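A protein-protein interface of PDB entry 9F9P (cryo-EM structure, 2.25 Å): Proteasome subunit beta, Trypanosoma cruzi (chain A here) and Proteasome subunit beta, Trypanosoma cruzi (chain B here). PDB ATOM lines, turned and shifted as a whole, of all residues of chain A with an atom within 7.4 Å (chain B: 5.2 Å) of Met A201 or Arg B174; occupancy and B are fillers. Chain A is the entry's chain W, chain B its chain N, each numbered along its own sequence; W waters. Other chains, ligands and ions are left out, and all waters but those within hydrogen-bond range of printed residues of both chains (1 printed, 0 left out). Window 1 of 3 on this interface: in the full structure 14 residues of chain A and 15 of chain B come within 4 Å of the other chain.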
ATOM      1  N   THR A  68      26.810  10.382  -3.622  1.00  0.00           N
ATOM      2  CA  THR A  68      25.419  10.641  -3.904  1.00  0.00           C
ATOM      3  C   THR A  68      24.604  10.270  -2.658  1.00  0.00           C
ATOM      4  O   THR A  68      24.732   9.157  -2.219  1.00  0.00           O
ATOM      5  CB  THR A  68      25.053   9.844  -5.172  1.00  0.00           C
ATOM      6  OG1 THR A  68      25.973  10.115  -6.231  1.00  0.00           O
ATOM      7  CG2 THR A  68      23.663  10.144  -5.683  1.00  0.00           C
ATOM      8  N   VAL A  70      20.454  10.608  -0.979  1.00  0.00           N
ATOM      9  CA  VAL A  70      19.071  10.805  -1.396  1.00  0.00           C
ATOM     10  C   VAL A  70      18.062  10.529  -0.267  1.00  0.00           C
ATOM     11  O   VAL A  70      18.192   9.567   0.446  1.00  0.00           O
ATOM     12  CB  VAL A  70      18.793   9.909  -2.609  1.00  0.00           C
ATOM     13  CG1 VAL A  70      17.344   9.806  -2.946  1.00  0.00           C
ATOM     14  CG2 VAL A  70      19.486  10.447  -3.829  1.00  0.00           C
ATOM     15  N   LEU A 188      11.509  19.197   2.773  1.00  0.00           N
ATOM     16  CA  LEU A 188      10.919  18.873   1.459  1.00  0.00           C
ATOM     17  C   LEU A 188      10.514  17.423   1.407  1.00  0.00           C
ATOM     18  O   LEU A 188      11.010  16.648   2.176  1.00  0.00           O
ATOM     19  CB  LEU A 188      11.922  19.142   0.321  1.00  0.00           C
ATOM     20  CG  LEU A 188      12.293  20.620   0.069  1.00  0.00           C
ATOM     21  CD1 LEU A 188      13.602  20.798  -0.710  1.00  0.00           C
ATOM     22  CD2 LEU A 188      11.177  21.337  -0.670  1.00  0.00           C
ATOM     23  N   PHE A 190      11.346  15.221  -1.203  1.00  0.00           N
ATOM     24  CA  PHE A 190      12.423  14.443  -1.815  1.00  0.00           C
ATOM     25  C   PHE A 190      13.627  15.357  -1.969  1.00  0.00           C
ATOM     26  O   PHE A 190      13.436  16.509  -2.267  1.00  0.00           O
ATOM     27  CB  PHE A 190      11.959  13.839  -3.142  1.00  0.00           C
ATOM     28  CG  PHE A 190      11.481  14.797  -4.209  1.00  0.00           C
ATOM     29  CD1 PHE A 190      10.140  15.136  -4.308  1.00  0.00           C
ATOM     30  CD2 PHE A 190      12.354  15.341  -5.143  1.00  0.00           C
ATOM     31  CE1 PHE A 190       9.677  16.038  -5.274  1.00  0.00           C
ATOM     32  CE2 PHE A 190      11.899  16.219  -6.127  1.00  0.00           C
ATOM     33  CZ  PHE A 190      10.564  16.577  -6.187  1.00  0.00           C
ATOM     34  N   VAL A 191      14.832  14.872  -1.679  1.00  0.00           N
ATOM     35  CA  VAL A 191      16.032  15.686  -1.757  1.00  0.00           C
ATOM     36  C   VAL A 191      17.171  14.848  -2.281  1.00  0.00           C
ATOM     37  O   VAL A 191      17.105  13.646  -2.203  1.00  0.00           O
ATOM     38  CB  VAL A 191      16.446  16.265  -0.386  1.00  0.00           C
ATOM     39  CG1 VAL A 191      15.341  17.055   0.240  1.00  0.00           C
ATOM     40  CG2 VAL A 191      16.814  15.201   0.624  1.00  0.00           C
ATOM     41  N   SER A 192      18.246  15.534  -2.682  1.00  0.00           N
ATOM     42  CA  SER A 192      19.526  14.929  -2.978  1.00  0.00           C
ATOM     43  C   SER A 192      20.663  15.905  -2.722  1.00  0.00           C
ATOM     44  O   SER A 192      20.514  17.086  -2.873  1.00  0.00           O
ATOM     45  CB  SER A 192      19.599  14.384  -4.401  1.00  0.00           C
ATOM     46  OG  SER A 192      19.630  15.409  -5.375  1.00  0.00           O
ATOM     47  N   MET A 193      21.812  15.371  -2.344  1.00  0.00           N
ATOM     48  CA  MET A 193      23.018  16.132  -2.130  1.00  0.00           C
ATOM     49  C   MET A 193      24.239  15.328  -2.563  1.00  0.00           C
ATOM     50  O   MET A 193      24.159  14.143  -2.839  1.00  0.00           O
ATOM     51  CB  MET A 193      23.188  16.466  -0.652  1.00  0.00           C
ATOM     52  CG  MET A 193      22.153  17.422  -0.135  1.00  0.00           C
ATOM     53  SD  MET A 193      22.564  18.006   1.512  1.00  0.00           S
ATOM     54  CE  MET A 193      22.655  19.770   1.190  1.00  0.00           C
ATOM     55  N   GLY A 196      27.016  13.734  -7.034  1.00  0.00           N
ATOM     56  CA  GLY A 196      26.027  13.100  -7.901  1.00  0.00           C
ATOM     57  C   GLY A 196      24.599  13.649  -7.766  1.00  0.00           C
ATOM     58  O   GLY A 196      23.678  13.042  -8.285  1.00  0.00           O
ATOM     59  N   SER A 197      24.381  14.752  -7.059  1.00  0.00           N
ATOM     60  CA  SER A 197      23.026  15.181  -6.753  1.00  0.00           C
ATOM     61  C   SER A 197      22.196  15.560  -7.984  1.00  0.00           C
ATOM     62  O   SER A 197      21.007  15.335  -7.987  1.00  0.00           O
ATOM     63  CB  SER A 197      23.010  16.321  -5.745  1.00  0.00           C
ATOM     64  OG  SER A 197      23.697  17.481  -6.207  1.00  0.00           O
ATOM     65  N   ILE A 198      22.789  16.167  -9.017  1.00  0.00           N
ATOM     66  CA  ILE A 198      22.022  16.558 -10.192  1.00  0.00           C
ATOM     67  C   ILE A 198      21.535  15.319 -10.955  1.00  0.00           C
ATOM     68  O   ILE A 198      20.389  15.237 -11.315  1.00  0.00           O
ATOM     69  CB  ILE A 198      22.843  17.493 -11.088  1.00  0.00           C
ATOM     70  CG1 ILE A 198      23.196  18.782 -10.369  1.00  0.00           C
ATOM     71  CG2 ILE A 198      22.132  17.806 -12.404  1.00  0.00           C
ATOM     72  CD1 ILE A 198      24.100  19.651 -11.196  1.00  0.00           C
ATOM     73  N   ALA A 199      22.375  14.336 -11.176  1.00  0.00           N
ATOM     74  CA  ALA A 199      21.920  13.127 -11.821  1.00  0.00           C
ATOM     75  C   ALA A 199      20.817  12.407 -11.052  1.00  0.00           C
ATOM     76  O   ALA A 199      19.893  11.880 -11.634  1.00  0.00           O
ATOM     77  CB  ALA A 199      23.087  12.214 -11.927  1.00  0.00           C
ATOM     78  N   ALA A 200      20.935  12.326  -9.723  1.00  0.00           N
ATOM     79  CA  ALA A 200      19.949  11.617  -8.916  1.00  0.00           C
ATOM     80  C   ALA A 200      18.617  12.344  -8.903  1.00  0.00           C
ATOM     81  O   ALA A 200      17.545  11.748  -8.880  1.00  0.00           O
ATOM     82  CB  ALA A 200      20.459  11.578  -7.514  1.00  0.00           C
ATOM     83  N   MET A 201      18.686  13.654  -8.915  1.00  0.00           N
ATOM     84  CA  MET A 201      17.490  14.461  -8.881  1.00  0.00           C
ATOM     85  C   MET A 201      16.724  14.347 -10.190  1.00  0.00           C
ATOM     86  O   MET A 201      15.536  14.659 -10.213  1.00  0.00           O
ATOM     87  CB  MET A 201      17.861  15.933  -8.666  1.00  0.00           C
ATOM     88  CG  MET A 201      16.656  16.896  -8.636  1.00  0.00           C
ATOM     89  SD  MET A 201      15.310  16.540  -7.419  1.00  0.00           S
ATOM     90  CE  MET A 201      16.157  16.973  -5.904  1.00  0.00           C
ATOM     91  N   SER A 202      17.391  13.925 -11.271  1.00  0.00           N
ATOM     92  CA  SER A 202      16.655  13.697 -12.507  1.00  0.00           C
ATOM     93  C   SER A 202      15.726  12.488 -12.412  1.00  0.00           C
ATOM     94  O   SER A 202      14.671  12.503 -12.978  1.00  0.00           O
ATOM     95  CB  SER A 202      17.570  13.646 -13.735  1.00  0.00           C
ATOM     96  OG  SER A 202      18.345  12.438 -13.760  1.00  0.00           O
ATOM     97  N   ALA A 203      16.107  11.423 -11.715  1.00  0.00           N
ATOM     98  CA  ALA A 203      15.201  10.304 -11.448  1.00  0.00           C
ATOM     99  C   ALA A 203      14.095  10.651 -10.454  1.00  0.00           C
ATOM    100  O   ALA A 203      13.020  10.100 -10.520  1.00  0.00           O
ATOM    101  CB  ALA A 203      16.012   9.181 -10.852  1.00  0.00           C
ATOM    102  N   LEU A 204      14.388  11.456  -9.436  1.00  0.00           N
ATOM    103  CA  LEU A 204      13.372  11.814  -8.452  1.00  0.00           C
ATOM    104  C   LEU A 204      12.227  12.625  -9.073  1.00  0.00           C
ATOM    105  O   LEU A 204      11.080  12.334  -8.813  1.00  0.00           O
ATOM    106  CB  LEU A 204      14.045  12.584  -7.317  1.00  0.00           C
ATOM    107  CG  LEU A 204      15.020  11.746  -6.481  1.00  0.00           C
ATOM    108  CD1 LEU A 204      15.670  12.610  -5.416  1.00  0.00           C
ATOM    109  CD2 LEU A 204      14.359  10.533  -5.850  1.00  0.00           C
ATOM    110  N   GLU A 205      12.552  13.648  -9.884  1.00  0.00           N
ATOM    111  CA  GLU A 205      11.529  14.437 -10.536  1.00  0.00           C
ATOM    112  C   GLU A 205      10.742  13.615 -11.568  1.00  0.00           C
ATOM    113  O   GLU A 205       9.602  13.935 -11.856  1.00  0.00           O
ATOM    114  CB  GLU A 205      12.108  15.649 -11.264  1.00  0.00           C
ATOM    115  CG  GLU A 205      12.666  16.728 -10.369  1.00  0.00           C
ATOM    116  CD  GLU A 205      11.703  17.736  -9.754  1.00  0.00           C
ATOM    117  OE1 GLU A 205      10.448  17.452  -9.727  1.00  0.00           O
ATOM    118  OE2 GLU A 205      12.199  18.809  -9.324  1.00  0.00           O
ATOM    119  N   THR A 206      11.303  12.567 -12.155  1.00  0.00           N
ATOM    120  CA  THR A 206      10.521  11.803 -13.123  1.00  0.00           C
ATOM    121  C   THR A 206       9.702  10.713 -12.433  1.00  0.00           C
ATOM    122  O   THR A 206       8.685  10.329 -12.967  1.00  0.00           O
ATOM    123  CB  THR A 206      11.427  11.244 -14.237  1.00  0.00           C
ATOM    124  OG1 THR A 206      12.738  10.877 -13.798  1.00  0.00           O
ATOM    125  CG2 THR A 206      11.775  12.301 -15.246  1.00  0.00           C
ATOM    126  N   GLY A 207      10.135  10.233 -11.253  1.00  0.00           N
ATOM    127  CA  GLY A 207       9.521   9.097 -10.596  1.00  0.00           C
ATOM    128  C   GLY A 207       8.688   9.360  -9.345  1.00  0.00           C
ATOM    129  O   GLY A 207       7.887   8.493  -8.987  1.00  0.00           O
ATOM    130  N   ALA A 224      17.579   6.363  -8.182  1.00  0.00           N
ATOM    131  CA  ALA A 224      18.309   7.610  -8.092  1.00  0.00           C
ATOM    132  C   ALA A 224      19.783   7.453  -7.725  1.00  0.00           C
ATOM    133  O   ALA A 224      20.596   8.198  -8.237  1.00  0.00           O
ATOM    134  CB  ALA A 224      17.642   8.521  -7.100  1.00  0.00           C
ATOM    135  N   LYS A 227      21.858   6.283 -10.828  1.00  0.00           N
ATOM    136  CA  LYS A 227      22.247   7.350 -11.730  1.00  0.00           C
ATOM    137  C   LYS A 227      23.548   8.041 -11.303  1.00  0.00           C
ATOM    138  O   LYS A 227      24.367   8.423 -12.126  1.00  0.00           O
ATOM    139  CB  LYS A 227      21.256   8.508 -11.763  1.00  0.00           C
ATOM    140  CG  LYS A 227      19.834   8.194 -12.187  1.00  0.00           C
ATOM    141  CD  LYS A 227      19.649   7.813 -13.587  1.00  0.00           C
ATOM    142  CE  LYS A 227      18.397   6.961 -13.737  1.00  0.00           C
ATOM    143  NZ  LYS A 227      18.659   5.545 -13.291  1.00  0.00           N
ATOM    144  N   VAL B 170      12.559  18.124 -16.694  1.00  0.00           N
ATOM    145  CA  VAL B 170      13.508  18.322 -15.630  1.00  0.00           C
ATOM    146  C   VAL B 170      14.369  19.555 -15.856  1.00  0.00           C
ATOM    147  O   VAL B 170      14.763  20.206 -14.879  1.00  0.00           O
ATOM    148  CB  VAL B 170      14.423  17.108 -15.437  1.00  0.00           C
ATOM    149  CG1 VAL B 170      15.336  17.334 -14.237  1.00  0.00           C
ATOM    150  CG2 VAL B 170      13.675  15.804 -15.224  1.00  0.00           C
ATOM    151  N   LEU B 171      14.727  19.882 -17.101  1.00  0.00           N
ATOM    152  CA  LEU B 171      15.536  21.082 -17.332  1.00  0.00           C
ATOM    153  C   LEU B 171      14.754  22.337 -16.951  1.00  0.00           C
ATOM    154  O   LEU B 171      15.309  23.258 -16.373  1.00  0.00           O
ATOM    155  CB  LEU B 171      15.973  21.169 -18.797  1.00  0.00           C
ATOM    156  CG  LEU B 171      17.066  20.191 -19.173  1.00  0.00           C
ATOM    157  CD1 LEU B 171      17.277  20.098 -20.670  1.00  0.00           C
ATOM    158  CD2 LEU B 171      18.359  20.614 -18.505  1.00  0.00           C
ATOM    159  N   PHE B 172      13.482  22.364 -17.229  1.00  0.00           N
ATOM    160  CA  PHE B 172      12.672  23.493 -16.846  1.00  0.00           C
ATOM    161  C   PHE B 172      12.514  23.614 -15.324  1.00  0.00           C
ATOM    162  O   PHE B 172      12.500  24.726 -14.799  1.00  0.00           O
ATOM    163  CB  PHE B 172      11.318  23.405 -17.546  1.00  0.00           C
ATOM    164  CG  PHE B 172      10.384  24.524 -17.192  1.00  0.00           C
ATOM    165  CD1 PHE B 172      10.719  25.845 -17.460  1.00  0.00           C
ATOM    166  CD2 PHE B 172       9.180  24.263 -16.536  1.00  0.00           C
ATOM    167  CE1 PHE B 172       9.857  26.873 -17.076  1.00  0.00           C
ATOM    168  CE2 PHE B 172       8.334  25.299 -16.138  1.00  0.00           C
ATOM    169  CZ  PHE B 172       8.650  26.602 -16.441  1.00  0.00           C
ATOM    170  N   TYR B 173      12.350  22.490 -14.611  1.00  0.00           N
ATOM    171  CA  TYR B 173      12.343  22.539 -13.147  1.00  0.00           C
ATOM    172  C   TYR B 173      13.683  22.981 -12.557  1.00  0.00           C
ATOM    173  O   TYR B 173      13.656  23.733 -11.609  1.00  0.00           O
ATOM    174  CB  TYR B 173      12.087  21.180 -12.508  1.00  0.00           C
ATOM    175  CG  TYR B 173      10.730  20.568 -12.700  1.00  0.00           C
ATOM    176  CD1 TYR B 173       9.576  21.288 -12.634  1.00  0.00           C
ATOM    177  CD2 TYR B 173      10.609  19.206 -12.835  1.00  0.00           C
ATOM    178  CE1 TYR B 173       8.325  20.700 -12.748  1.00  0.00           C
ATOM    179  CE2 TYR B 173       9.381  18.601 -12.995  1.00  0.00           C
ATOM    180  CZ  TYR B 173       8.233  19.348 -12.924  1.00  0.00           C
ATOM    181  OH  TYR B 173       7.054  18.674 -13.072  1.00  0.00           O
ATOM    182  N   ARG B 174      14.836  22.594 -13.123  1.00  0.00           N
ATOM    183  CA  ARG B 174      16.099  22.700 -12.401  1.00  0.00           C
ATOM    184  C   ARG B 174      17.186  23.553 -13.042  1.00  0.00           C
ATOM    185  O   ARG B 174      18.131  23.882 -12.342  1.00  0.00           O
ATOM    186  CB  ARG B 174      16.656  21.301 -12.126  1.00  0.00           C
ATOM    187  CG  ARG B 174      15.712  20.370 -11.347  1.00  0.00           C
ATOM    188  CD  ARG B 174      15.725  20.750  -9.879  1.00  0.00           C
ATOM    189  NE  ARG B 174      14.672  20.189  -9.057  1.00  0.00           N
ATOM    190  CZ  ARG B 174      14.652  20.285  -7.721  1.00  0.00           C
ATOM    191  NH1 ARG B 174      15.680  20.818  -7.077  1.00  0.00           N
ATOM    192  NH2 ARG B 174      13.647  19.782  -7.028  1.00  0.00           N
ATOM    193  N   GLU B 175      17.054  23.989 -14.296  1.00  0.00           N
ATOM    194  CA  GLU B 175      18.016  24.905 -14.924  1.00  0.00           C
ATOM    195  C   GLU B 175      17.458  26.315 -14.781  1.00  0.00           C
ATOM    196  O   GLU B 175      16.349  26.563 -15.173  1.00  0.00           O
ATOM    197  CB  GLU B 175      18.265  24.431 -16.378  1.00  0.00           C
ATOM    198  CG  GLU B 175      19.330  25.232 -17.174  1.00  0.00           C
ATOM    199  CD  GLU B 175      19.553  25.042 -18.705  1.00  0.00           C
ATOM    200  OE1 GLU B 175      18.661  24.469 -19.433  1.00  0.00           O
ATOM    201  OE2 GLU B 175      20.631  25.500 -19.219  1.00  0.00           O
ATOM    202  N   CYS B 176      18.160  27.252 -14.148  1.00  0.00           N
ATOM    203  CA  CYS B 176      17.608  28.591 -13.934  1.00  0.00           C
ATOM    204  C   CYS B 176      17.277  29.350 -15.220  1.00  0.00           C
ATOM    205  O   CYS B 176      16.191  29.926 -15.333  1.00  0.00           O
ATOM    206  CB  CYS B 176      18.581  29.498 -13.201  1.00  0.00           C
ATOM    207  SG  CYS B 176      18.818  28.991 -11.480  1.00  0.00           S
HETATM  208  O   HOH W   1      14.324  19.136  -3.937  1.00  0.00           O
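The side-chain sulfur (SD) of Met A201 sits at hydrogen-bond distance from the guanidinium group (NH2) of Arg B174, at 3.7 Å.
The side-chain carboxylate of Glu A205 is in salt-bridge range of the guanidinium group of Arg B174 (2.8 Å).
Among the printed residues, pairs that only touch across the chains: Glu A205 with Tyr B173 (3.6 Å) and Thr A206 with Val B170 (3.99 Å).
The backbone carbonyl oxygen (O) of Ser A202 lies within hydrogen-bond range of the side-chain hydroxyl (OG1) of Thr A206 (2.7 Å).
O of Ala A203 sits at hydrogen-bond distance from OG1 of Thr A206 (3.4 Å).
Water W1 lies within hydrogen-bond range of the guanidinium group of Arg B174 and the backbone carbonyl oxygen of Phe A190.
Of the printed residues of chain B, Met A201 touches Arg B174.
Of the printed residues of chain B, Glu A205 touches Tyr B173 (3.6 Å) and Arg B174 (2.8 Å).
Printed residues of chain B within 4 Å of Thr A206: Val B170 (3.99 Å).
Of the printed residues of chain A, Val B170 touches Thr A206 (3.99 Å).
Of the printed residues of chain A, Tyr B173 touches Glu A205.
Of chain A, only Met A201 and Glu A205 come within 4 Å of Arg B174.
The nearest residue of chain A that does not touch Arg B174 is Phe A190 (4.1 Å).
The nearest printed residue of chain B that does not touch Thr A206 is Tyr B173 (6.4 Å).
Hydrophobic or aromatic side chains of chain A that line the printed part of chain B: Met A201.
Printed residues of chain B that touch a printed residue of chain A: Val B170, Tyr B173 and Arg B174.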
